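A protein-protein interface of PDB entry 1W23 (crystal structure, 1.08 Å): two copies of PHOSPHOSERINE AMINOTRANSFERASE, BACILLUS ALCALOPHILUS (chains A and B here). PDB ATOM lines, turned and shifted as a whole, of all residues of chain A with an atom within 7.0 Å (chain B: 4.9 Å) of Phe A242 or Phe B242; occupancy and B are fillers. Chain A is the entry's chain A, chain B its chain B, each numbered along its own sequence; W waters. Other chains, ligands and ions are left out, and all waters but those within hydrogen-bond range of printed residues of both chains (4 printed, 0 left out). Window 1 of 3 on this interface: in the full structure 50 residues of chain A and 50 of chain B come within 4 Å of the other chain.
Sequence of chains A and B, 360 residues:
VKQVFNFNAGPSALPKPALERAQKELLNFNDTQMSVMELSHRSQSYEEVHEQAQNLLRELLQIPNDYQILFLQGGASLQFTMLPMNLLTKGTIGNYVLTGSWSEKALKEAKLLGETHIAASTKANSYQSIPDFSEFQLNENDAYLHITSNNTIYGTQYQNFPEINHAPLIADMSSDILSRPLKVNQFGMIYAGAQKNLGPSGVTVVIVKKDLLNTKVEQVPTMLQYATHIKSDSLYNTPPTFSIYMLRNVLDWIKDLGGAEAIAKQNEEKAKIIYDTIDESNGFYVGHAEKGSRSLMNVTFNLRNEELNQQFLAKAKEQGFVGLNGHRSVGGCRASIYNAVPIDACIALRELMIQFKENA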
ATOM      1  N   LEU A  19      14.427 -34.173  -8.397  1.00  0.00           N
ATOM      2  CA  LEU A  19      14.022 -32.783  -8.203  1.00  0.00           C
ATOM      3  C   LEU A  19      14.297 -32.331  -6.782  1.00  0.00           C
ATOM      4  O   LEU A  19      14.727 -31.173  -6.587  1.00  0.00           O
ATOM      5  CB  LEU A  19      12.542 -32.577  -8.575  1.00  0.00           C
ATOM      6  CG  LEU A  19      12.250 -32.563 -10.088  1.00  0.00           C
ATOM      7  CD1 LEU A  19      10.747 -32.751 -10.298  1.00  0.00           C
ATOM      8  CD2 LEU A  19      12.726 -31.284 -10.716  1.00  0.00           C
ATOM      9  N   ALA A  22      17.933 -31.701  -6.498  1.00  0.00           N
ATOM     10  CA  ALA A  22      18.303 -30.450  -7.169  1.00  0.00           C
ATOM     11  C   ALA A  22      17.874 -29.233  -6.348  1.00  0.00           C
ATOM     12  O   ALA A  22      18.597 -28.225  -6.261  1.00  0.00           O
ATOM     13  CB  ALA A  22      17.631 -30.412  -8.542  1.00  0.00           C
ATOM     14  N   GLN A  23      16.674 -29.268  -5.768  1.00  0.00           N
ATOM     15  CA  GLN A  23      16.180 -28.162  -4.958  1.00  0.00           C
ATOM     16  C   GLN A  23      17.128 -27.901  -3.773  1.00  0.00           C
ATOM     17  O   GLN A  23      17.487 -26.764  -3.498  1.00  0.00           O
ATOM     18  CB  GLN A  23      14.778 -28.452  -4.464  1.00  0.00           C
ATOM     19  CG  GLN A  23      14.157 -27.301  -3.682  1.00  0.00           C
ATOM     20  CD  GLN A  23      12.796 -27.654  -3.147  1.00  0.00           C
ATOM     21  OE1 GLN A  23      12.575 -28.744  -2.570  1.00  0.00           O
ATOM     22  NE2 GLN A  23      11.824 -26.785  -3.322  1.00  0.00           N
ATOM     23  N   LEU A  26      20.434 -26.275  -4.900  1.00  0.00           N
ATOM     24  CA  LEU A  26      20.348 -25.332  -6.032  1.00  0.00           C
ATOM     25  C   LEU A  26      21.260 -24.138  -5.832  1.00  0.00           C
ATOM     26  O   LEU A  26      21.694 -23.569  -6.837  1.00  0.00           O
ATOM     27  CB  LEU A  26      18.916 -24.860  -6.288  1.00  0.00           C
ATOM     28  CG  LEU A  26      18.688 -24.377  -7.706  1.00  0.00           C
ATOM     29  CD1 LEU A  26      18.650 -25.506  -8.701  1.00  0.00           C
ATOM     30  CD2 LEU A  26      17.371 -23.577  -7.813  1.00  0.00           C
ATOM     31  N   SER A  35      25.535 -22.289  -7.408  1.00  0.00           N
ATOM     32  CA  SER A  35      24.685 -23.270  -8.094  1.00  0.00           C
ATOM     33  C   SER A  35      25.464 -24.025  -9.143  1.00  0.00           C
ATOM     34  O   SER A  35      26.415 -23.460  -9.730  1.00  0.00           O
ATOM     35  CB  SER A  35      23.553 -22.510  -8.799  1.00  0.00           C
ATOM     36  OG  SER A  35      22.657 -23.407  -9.442  1.00  0.00           O
ATOM     37  N   VAL A  36      25.038 -25.243  -9.465  1.00  0.00           N
ATOM     38  CA  VAL A  36      25.631 -25.919 -10.639  1.00  0.00           C
ATOM     39  C   VAL A  36      25.480 -24.995 -11.853  1.00  0.00           C
ATOM     40  O   VAL A  36      26.352 -25.053 -12.724  1.00  0.00           O
ATOM     41  CB  VAL A  36      25.060 -27.371 -10.756  1.00  0.00           C
ATOM     42  CG1 VAL A  36      23.656 -27.268 -11.188  1.00  0.00           C
ATOM     43  CG2 VAL A  36      25.921 -28.195 -11.671  1.00  0.00           C
ATOM     44  N   MET A  37      24.420 -24.172 -11.958  1.00  0.00           N
ATOM     45  CA  MET A  37      24.132 -23.203 -13.058  1.00  0.00           C
ATOM     46  C   MET A  37      25.132 -22.090 -13.131  1.00  0.00           C
ATOM     47  O   MET A  37      25.119 -21.361 -14.129  1.00  0.00           O
ATOM     48  CB  MET A  37      22.697 -22.615 -12.902  1.00  0.00           C
ATOM     49  CG  MET A  37      21.590 -23.441 -13.437  1.00  0.00           C
ATOM     50  SD  MET A  37      20.161 -22.482 -13.100  1.00  0.00           S
ATOM     51  CE  MET A  37      19.640 -23.316 -11.673  1.00  0.00           C
ATOM     52  N   TYR A  46      31.794 -29.502 -12.026  1.00  0.00           N
ATOM     53  CA  TYR A  46      30.970 -29.776 -13.215  1.00  0.00           C
ATOM     54  C   TYR A  46      31.549 -30.994 -13.955  1.00  0.00           C
ATOM     55  O   TYR A  46      30.811 -31.858 -14.428  1.00  0.00           O
ATOM     56  CB  TYR A  46      30.734 -28.527 -14.137  1.00  0.00           C
ATOM     57  CG  TYR A  46      29.917 -29.093 -15.285  1.00  0.00           C
ATOM     58  CD1 TYR A  46      28.557 -29.329 -15.119  1.00  0.00           C
ATOM     59  CD2 TYR A  46      30.487 -29.421 -16.539  1.00  0.00           C
ATOM     60  CE1 TYR A  46      27.797 -29.859 -16.177  1.00  0.00           C
ATOM     61  CE2 TYR A  46      29.732 -29.957 -17.556  1.00  0.00           C
ATOM     62  CZ  TYR A  46      28.385 -30.168 -17.361  1.00  0.00           C
ATOM     63  OH  TYR A  46      27.600 -30.711 -18.380  1.00  0.00           O
ATOM     64  N   PRO A 200      15.261 -33.310 -18.086  1.00  0.00           N
ATOM     65  CA  PRO A 200      14.545 -32.183 -18.670  1.00  0.00           C
ATOM     66  C   PRO A 200      15.066 -31.925 -20.100  1.00  0.00           C
ATOM     67  O   PRO A 200      15.932 -32.478 -20.646  1.00  0.00           O
ATOM     68  CB  PRO A 200      14.785 -31.012 -17.698  1.00  0.00           C
ATOM     69  CG  PRO A 200      16.192 -31.271 -17.232  1.00  0.00           C
ATOM     70  CD  PRO A 200      16.170 -32.775 -17.008  1.00  0.00           C
ATOM     71  N   SER A 201      14.322 -31.037 -20.730  1.00  0.00           N
ATOM     72  CA  SER A 201      14.694 -30.596 -22.068  1.00  0.00           C
ATOM     73  C   SER A 201      15.942 -29.775 -22.097  1.00  0.00           C
ATOM     74  O   SER A 201      16.325 -29.182 -21.091  1.00  0.00           O
ATOM     75  CB  SER A 201      13.511 -29.795 -22.653  1.00  0.00           C
ATOM     76  OG  SER A 201      13.425 -28.570 -21.962  1.00  0.00           O
ATOM     77  N   PRO A 239      28.272 -26.379 -22.659  1.00  0.00           N
ATOM     78  CA  PRO A 239      27.163 -27.359 -22.646  1.00  0.00           C
ATOM     79  C   PRO A 239      25.980 -26.832 -21.842  1.00  0.00           C
ATOM     80  O   PRO A 239      26.126 -25.880 -21.080  1.00  0.00           O
ATOM     81  CB  PRO A 239      27.788 -28.565 -21.995  1.00  0.00           C
ATOM     82  CG  PRO A 239      28.846 -27.997 -21.084  1.00  0.00           C
ATOM     83  CD  PRO A 239      29.371 -26.775 -21.767  1.00  0.00           C
ATOM     84  N   PRO A 240      24.848 -27.493 -21.974  1.00  0.00           N
ATOM     85  CA  PRO A 240      23.649 -27.208 -21.155  1.00  0.00           C
ATOM     86  C   PRO A 240      23.857 -27.851 -19.769  1.00  0.00           C
ATOM     87  O   PRO A 240      23.414 -28.969 -19.502  1.00  0.00           O
ATOM     88  CB  PRO A 240      22.521 -27.816 -21.973  1.00  0.00           C
ATOM     89  CG  PRO A 240      23.164 -28.996 -22.653  1.00  0.00           C
ATOM     90  CD  PRO A 240      24.555 -28.523 -22.994  1.00  0.00           C
ATOM     91  N   THR A 241      24.577 -27.145 -18.903  1.00  0.00           N
ATOM     92  CA  THR A 241      25.109 -27.772 -17.689  1.00  0.00           C
ATOM     93  C   THR A 241      23.999 -28.203 -16.729  1.00  0.00           C
ATOM     94  O   THR A 241      24.084 -29.289 -16.164  1.00  0.00           O
ATOM     95  CB  THR A 241      26.089 -26.831 -16.960  1.00  0.00           C
ATOM     96  OG1 THR A 241      25.441 -25.574 -16.746  1.00  0.00           O
ATOM     97  CG2 THR A 241      27.377 -26.620 -17.723  1.00  0.00           C
ATOM     98  N   PHE A 242      22.975 -27.382 -16.565  1.00  0.00           N
ATOM     99  CA  PHE A 242      21.893 -27.761 -15.631  1.00  0.00           C
ATOM    100  C   PHE A 242      21.113 -28.953 -16.189  1.00  0.00           C
ATOM    101  O   PHE A 242      20.746 -29.876 -15.423  1.00  0.00           O
ATOM    102  CB  PHE A 242      20.977 -26.599 -15.291  1.00  0.00           C
ATOM    103  CG  PHE A 242      20.039 -26.941 -14.131  1.00  0.00           C
ATOM    104  CD1 PHE A 242      20.542 -27.057 -12.846  1.00  0.00           C
ATOM    105  CD2 PHE A 242      18.702 -27.139 -14.327  1.00  0.00           C
ATOM    106  CE1 PHE A 242      19.711 -27.381 -11.805  1.00  0.00           C
ATOM    107  CE2 PHE A 242      17.861 -27.467 -13.266  1.00  0.00           C
ATOM    108  CZ  PHE A 242      18.366 -27.565 -11.973  1.00  0.00           C
ATOM    109  N   SER A 243      20.870 -28.995 -17.480  1.00  0.00           N
ATOM    110  CA  SER A 243      20.171 -30.160 -18.071  1.00  0.00           C
ATOM    111  C   SER A 243      20.994 -31.428 -17.894  1.00  0.00           C
ATOM    112  O   SER A 243      20.398 -32.500 -17.597  1.00  0.00           O
ATOM    113  CB  SER A 243      19.839 -29.922 -19.534  1.00  0.00           C
ATOM    114  OG  SER A 243      18.926 -28.874 -19.693  1.00  0.00           O
ATOM    115  N   ILE A 244      22.296 -31.375 -18.086  1.00  0.00           N
ATOM    116  CA  ILE A 244      23.136 -32.567 -17.908  1.00  0.00           C
ATOM    117  C   ILE A 244      23.197 -32.970 -16.448  1.00  0.00           C
ATOM    118  O   ILE A 244      23.167 -34.183 -16.116  1.00  0.00           O
ATOM    119  CB  ILE A 244      24.527 -32.335 -18.550  1.00  0.00           C
ATOM    120  CG1 ILE A 244      24.389 -32.246 -20.075  1.00  0.00           C
ATOM    121  CG2 ILE A 244      25.508 -33.411 -18.128  1.00  0.00           C
ATOM    122  CD1 ILE A 244      25.554 -31.597 -20.801  1.00  0.00           C
ATOM    123  N   TYR A 245      23.249 -32.013 -15.531  1.00  0.00           N
ATOM    124  CA  TYR A 245      23.183 -32.315 -14.094  1.00  0.00           C
ATOM    125  C   TYR A 245      21.867 -32.986 -13.768  1.00  0.00           C
ATOM    126  O   TYR A 245      21.842 -34.005 -13.027  1.00  0.00           O
ATOM    127  CB  TYR A 245      23.347 -30.965 -13.342  1.00  0.00           C
ATOM    128  CG  TYR A 245      22.850 -31.027 -11.931  1.00  0.00           C
ATOM    129  CD1 TYR A 245      23.622 -31.532 -10.886  1.00  0.00           C
ATOM    130  CD2 TYR A 245      21.572 -30.583 -11.595  1.00  0.00           C
ATOM    131  CE1 TYR A 245      23.135 -31.574  -9.592  1.00  0.00           C
ATOM    132  CE2 TYR A 245      21.085 -30.657 -10.326  1.00  0.00           C
ATOM    133  CZ  TYR A 245      21.891 -31.160  -9.310  1.00  0.00           C
ATOM    134  OH  TYR A 245      21.345 -31.227  -8.047  1.00  0.00           O
ATOM    135  N   MET A 246      20.734 -32.495 -14.283  1.00  0.00           N
ATOM    136  CA  MET A 246      19.451 -33.151 -13.991  1.00  0.00           C
ATOM    137  C   MET A 246      19.408 -34.543 -14.584  1.00  0.00           C
ATOM    138  O   MET A 246      18.853 -35.470 -13.951  1.00  0.00           O
ATOM    139  CB  MET A 246      18.289 -32.293 -14.498  1.00  0.00           C
ATOM    140  CG  MET A 246      18.022 -31.076 -13.658  1.00  0.00           C
ATOM    141  SD  MET A 246      17.566 -31.401 -11.969  1.00  0.00           S
ATOM    142  CE  MET A 246      16.218 -32.526 -12.116  1.00  0.00           C
ATOM    143  N   LEU A 247      19.930 -34.749 -15.797  1.00  0.00           N
ATOM    144  CA  LEU A 247      20.063 -36.051 -16.397  1.00  0.00           C
ATOM    145  C   LEU A 247      20.848 -36.989 -15.459  1.00  0.00           C
ATOM    146  O   LEU A 247      20.416 -38.126 -15.204  1.00  0.00           O
ATOM    147  CB  LEU A 247      20.755 -35.915 -17.762  1.00  0.00           C
ATOM    148  CG  LEU A 247      21.224 -37.213 -18.445  1.00  0.00           C
ATOM    149  CD1 LEU A 247      20.168 -38.127 -18.829  1.00  0.00           C
ATOM    150  CD2 LEU A 247      22.129 -36.821 -19.624  1.00  0.00           C
ATOM    151  N   ARG A 248      21.988 -36.534 -14.931  1.00  0.00           N
ATOM    152  CA  ARG A 248      22.729 -37.328 -13.977  1.00  0.00           C
ATOM    153  C   ARG A 248      21.819 -37.739 -12.829  1.00  0.00           C
ATOM    154  O   ARG A 248      21.804 -38.915 -12.419  1.00  0.00           O
ATOM    155  CB  ARG A 248      23.971 -36.519 -13.538  1.00  0.00           C
ATOM    156  CG  ARG A 248      25.010 -37.305 -12.719  1.00  0.00           C
ATOM    157  CD  ARG A 248      24.624 -37.661 -11.268  1.00  0.00           C
ATOM    158  NE  ARG A 248      24.206 -36.455 -10.509  1.00  0.00           N
ATOM    159  CZ  ARG A 248      25.050 -35.704  -9.846  1.00  0.00           C
ATOM    160  NH1 ARG A 248      26.347 -35.991  -9.744  1.00  0.00           N
ATOM    161  NH2 ARG A 248      24.584 -34.585  -9.241  1.00  0.00           N
ATOM    162  N   ALA B  22      13.640 -19.696  -8.002  1.00  0.00           N
ATOM    163  CA  ALA B  22      13.638 -20.998  -8.687  1.00  0.00           C
ATOM    164  C   ALA B  22      13.652 -22.135  -7.684  1.00  0.00           C
ATOM    165  O   ALA B  22      12.931 -23.134  -7.841  1.00  0.00           O
ATOM    166  CB  ALA B  22      14.813 -21.090  -9.618  1.00  0.00           C
ATOM    167  N   LEU B  26      10.644 -25.034  -7.243  1.00  0.00           N
ATOM    168  CA  LEU B  26      11.187 -26.055  -8.119  1.00  0.00           C
ATOM    169  C   LEU B  26      10.256 -27.265  -8.269  1.00  0.00           C
ATOM    170  O   LEU B  26      10.277 -27.938  -9.288  1.00  0.00           O
ATOM    171  CB  LEU B  26      12.584 -26.509  -7.682  1.00  0.00           C
ATOM    172  CG  LEU B  26      13.424 -27.107  -8.813  1.00  0.00           C
ATOM    173  CD1 LEU B  26      13.947 -26.030  -9.728  1.00  0.00           C
ATOM    174  CD2 LEU B  26      14.592 -27.893  -8.276  1.00  0.00           C
ATOM    175  N   VAL B  36       8.474 -26.559 -13.271  1.00  0.00           N
ATOM    176  CA  VAL B  36       8.505 -26.020 -14.631  1.00  0.00           C
ATOM    177  C   VAL B  36       9.154 -27.028 -15.570  1.00  0.00           C
ATOM    178  O   VAL B  36       8.764 -27.059 -16.764  1.00  0.00           O
ATOM    179  CB  VAL B  36       9.077 -24.581 -14.578  1.00  0.00           C
ATOM    180  CG1 VAL B  36      10.543 -24.655 -14.425  1.00  0.00           C
ATOM    181  CG2 VAL B  36       8.699 -23.790 -15.822  1.00  0.00           C
ATOM    182  N   MET B  37      10.095 -27.856 -15.121  1.00  0.00           N
ATOM    183  CA  MET B  37      10.752 -28.900 -15.908  1.00  0.00           C
ATOM    184  C   MET B  37       9.860 -30.056 -16.318  1.00  0.00           C
ATOM    185  O   MET B  37      10.304 -30.898 -17.123  1.00  0.00           O
ATOM    186  CB  MET B  37      11.946 -29.493 -15.082  1.00  0.00           C
ATOM    187  CG  MET B  37      13.168 -28.638 -15.093  1.00  0.00           C
ATOM    188  SD  MET B  37      14.487 -29.396 -14.144  1.00  0.00           S
ATOM    189  CE  MET B  37      14.272 -28.570 -12.632  1.00  0.00           C
ATOM    190  N   PRO B 240      14.374 -25.261 -24.597  1.00  0.00           N
ATOM    191  CA  PRO B 240      15.037 -25.471 -23.301  1.00  0.00           C
ATOM    192  C   PRO B 240      14.254 -24.764 -22.220  1.00  0.00           C
ATOM    193  O   PRO B 240      14.503 -23.613 -21.854  1.00  0.00           O
ATOM    194  CB  PRO B 240      16.433 -24.884 -23.540  1.00  0.00           C
ATOM    195  CG  PRO B 240      16.206 -23.788 -24.517  1.00  0.00           C
ATOM    196  CD  PRO B 240      15.133 -24.321 -25.473  1.00  0.00           C
ATOM    197  N   THR B 241      13.190 -25.434 -21.738  1.00  0.00           N
ATOM    198  CA  THR B 241      12.177 -24.772 -20.944  1.00  0.00           C
ATOM    199  C   THR B 241      12.716 -24.218 -19.645  1.00  0.00           C
ATOM    200  O   THR B 241      12.357 -23.084 -19.280  1.00  0.00           O
ATOM    201  CB  THR B 241      10.950 -25.709 -20.709  1.00  0.00           C
ATOM    202  OG1 THR B 241      11.458 -26.907 -20.090  1.00  0.00           O
ATOM    203  CG2 THR B 241      10.207 -26.071 -21.977  1.00  0.00           C
ATOM    204  N   PHE B 242      13.522 -24.971 -18.920  1.00  0.00           N
ATOM    205  CA  PHE B 242      14.048 -24.443 -17.646  1.00  0.00           C
ATOM    206  C   PHE B 242      14.984 -23.271 -17.874  1.00  0.00           C
ATOM    207  O   PHE B 242      14.975 -22.305 -17.113  1.00  0.00           O
ATOM    208  CB  PHE B 242      14.737 -25.547 -16.839  1.00  0.00           C
ATOM    209  CG  PHE B 242      15.045 -25.076 -15.442  1.00  0.00           C
ATOM    210  CD1 PHE B 242      14.064 -24.943 -14.483  1.00  0.00           C
ATOM    211  CD2 PHE B 242      16.324 -24.734 -15.071  1.00  0.00           C
ATOM    212  CE1 PHE B 242      14.380 -24.482 -13.238  1.00  0.00           C
ATOM    213  CE2 PHE B 242      16.636 -24.328 -13.826  1.00  0.00           C
ATOM    214  CZ  PHE B 242      15.649 -24.174 -12.876  1.00  0.00           C
ATOM    215  N   SER B 243      15.818 -23.334 -18.937  1.00  0.00           N
ATOM    216  CA  SER B 243      16.686 -22.212 -19.210  1.00  0.00           C
ATOM    217  C   SER B 243      15.906 -20.939 -19.528  1.00  0.00           C
ATOM    218  O   SER B 243      16.286 -19.852 -19.129  1.00  0.00           O
ATOM    219  CB  SER B 243      17.665 -22.535 -20.356  1.00  0.00           C
ATOM    220  OG  SER B 243      18.579 -23.518 -19.919  1.00  0.00           O
ATOM    221  N   ILE B 244      14.806 -21.066 -20.289  1.00  0.00           N
ATOM    222  CA  ILE B 244      13.959 -19.900 -20.601  1.00  0.00           C
ATOM    223  C   ILE B 244      13.235 -19.398 -19.372  1.00  0.00           C
ATOM    224  O   ILE B 244      13.122 -18.171 -19.171  1.00  0.00           O
ATOM    225  CB  ILE B 244      13.036 -20.245 -21.788  1.00  0.00           C
ATOM    226  CG1 ILE B 244      13.876 -20.426 -23.062  1.00  0.00           C
ATOM    227  CG2 ILE B 244      11.946 -19.173 -21.966  1.00  0.00           C
ATOM    228  CD1 ILE B 244      13.146 -21.189 -24.171  1.00  0.00           C
ATOM    229  N   TYR B 245      12.761 -20.291 -18.510  1.00  0.00           N
ATOM    230  CA  TYR B 245      12.216 -19.882 -17.214  1.00  0.00           C
ATOM    231  C   TYR B 245      13.254 -19.095 -16.409  1.00  0.00           C
ATOM    232  O   TYR B 245      12.928 -18.068 -15.812  1.00  0.00           O
ATOM    233  CB  TYR B 245      11.745 -21.165 -16.478  1.00  0.00           C
ATOM    234  CG  TYR B 245      11.564 -20.970 -14.995  1.00  0.00           C
ATOM    235  CD1 TYR B 245      10.408 -20.448 -14.448  1.00  0.00           C
ATOM    236  CD2 TYR B 245      12.577 -21.311 -14.125  1.00  0.00           C
ATOM    237  CE1 TYR B 245      10.266 -20.275 -13.101  1.00  0.00           C
ATOM    238  CE2 TYR B 245      12.456 -21.122 -12.763  1.00  0.00           C
ATOM    239  CZ  TYR B 245      11.282 -20.610 -12.247  1.00  0.00           C
ATOM    240  OH  TYR B 245      11.189 -20.413 -10.877  1.00  0.00           O
ATOM    241  N   MET B 246      14.493 -19.594 -16.335  1.00  0.00           N
ATOM    242  CA  MET B 246      15.527 -18.880 -15.583  1.00  0.00           C
ATOM    243  C   MET B 246      15.841 -17.524 -16.199  1.00  0.00           C
ATOM    244  O   MET B 246      16.050 -16.551 -15.468  1.00  0.00           O
ATOM    245  CB  MET B 246      16.789 -19.734 -15.438  1.00  0.00           C
ATOM    246  CG  MET B 246      16.690 -20.867 -14.464  1.00  0.00           C
ATOM    247  SD  MET B 246      16.329 -20.393 -12.780  1.00  0.00           S
ATOM    248  CE  MET B 246      17.583 -19.156 -12.485  1.00  0.00           C
HETATM  249  O   HOH W   1      11.989 -29.784 -19.262  1.00  0.00           O
HETATM  250  O   HOH W   2      14.344 -27.843 -19.326  1.00  0.00           O
HETATM  251  O   HOH W   3      16.385 -25.997 -20.223  1.00  0.00           O
HETATM  252  O   HOH W   4      19.042 -26.047 -21.204  1.00  0.00           O
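O of Leu A19 touches CD2 of Leu B26 (3.7 Å).
CB of Ala A22 touches CD2 of Leu B26, at 3.96 Å.
Leu B26 touches Gln A23 (CD2 to N, 3.5 Å).
Leu A26 touches Ala B22 (CD2 to C, 3.99 Å).
Met A37 touches Phe B242.
Pro A200 touches Met B37.
Pro B240 touches Ser A201.
CE of Met B37 touches CE2 of Phe A242, at 3.8 Å.
Phe A242 touches Phe B242.
Met B37 touches Met A246 (SD to CG, 3.9 Å).
Of the 20 printed residues of chain A, 9 touch a printed residue of chain B.
Hydrophobic or aromatic side chains of chain A that line the printed part of chain B: Leu A19, Ala A22, Leu A26, Met A37, Pro A200, Phe A242 and Met A246.
Of the 11 printed residues of chain B, 6 touch a printed residue of chain A.
Hydrophobic or aromatic side chains of chain B that line the printed part of chain A: Ala B22, Leu B26, Met B37 and Phe B242.
Among the printed residues, 12 pairs touch across the chains.
Ala A22 touches Leu B26, and with the chains exchanged Leu A26 touches Ala B22.
Met A37 touches Phe B242, and with the chains exchanged Phe A242 touches Met B37.
Phe B242 touches its own counterpart, Phe A242.
Met A246 touches Met B37, but with the chains exchanged Met A37 does not touch Met B246 (4.1 Å).
Positions printed for both chains: 22, 26, 36, 37, 240, 241, 242, 243, 244, 245 and 246.
Of the printed residues of chain B, Ala A22 touches Leu B26 (3.96 Å).
Printed residues of chain B within 4 Å of Gln A23: Leu B26.
Printed residues of chain B within 4 Å of Leu A26: Ala B22.
Of the printed residues of chain B, Pro A200 touches Met B37 (3.9 Å).
Phe A242 touches just these residues of chain B: Met B37 (3.8 Å) and Phe B242 (3.4 Å).
Ser A243 touches none of the printed residues of chain B.
Arg A248 touches none of the printed residues of chain B.
Of the printed residues of chain A, Thr B241 touches Ser A201 (3.2 Å).
Printed residues of chain A within 4 Å of Phe B242: Met A37 and Phe A242.
The nearest printed residue of chain B that does not touch Phe A242 is Leu B26 (5.2 Å).
The nearest residue of chain A that does not touch Phe B242 is Ser A201 (4.7 Å).
Water W4 lies within hydrogen-bond range of the side-chain hydroxyl of Ser B243 (2.9 Å) and the side-chain hydroxyl of Ser A243 (3.2 Å).
Water W2 lies within hydrogen-bond range of OG of Ser A201, N of Phe B242 and OG1 of Thr B241.
Water W1 lies within hydrogen-bond range of O of Met B37, N of Ser A201 and OG1 of Thr B241.
Water W3 lies within hydrogen-bond range of N of Ser B243 (3.0 Å), O of Ser A201 (3.3 Å), N of Phe B242 (3.3 Å) and O of Pro B240 (3.4 Å).
OG of Ser A201 is in hydrogen-bond range of N of Thr B241.
The backbone carbonyl oxygen (O) of Leu A26 lies within hydrogen-bond range of the side-chain hydroxyl (OG) of Ser A35, 2.8 Å away.
The backbone NH of Met A37 lies close to the side-chain hydroxyl of Ser A35, 3.2 Å away.
The backbone carbonyl oxygen of Ser A201 is in hydrogen-bond range of the side-chain hydroxyl of Ser A243.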
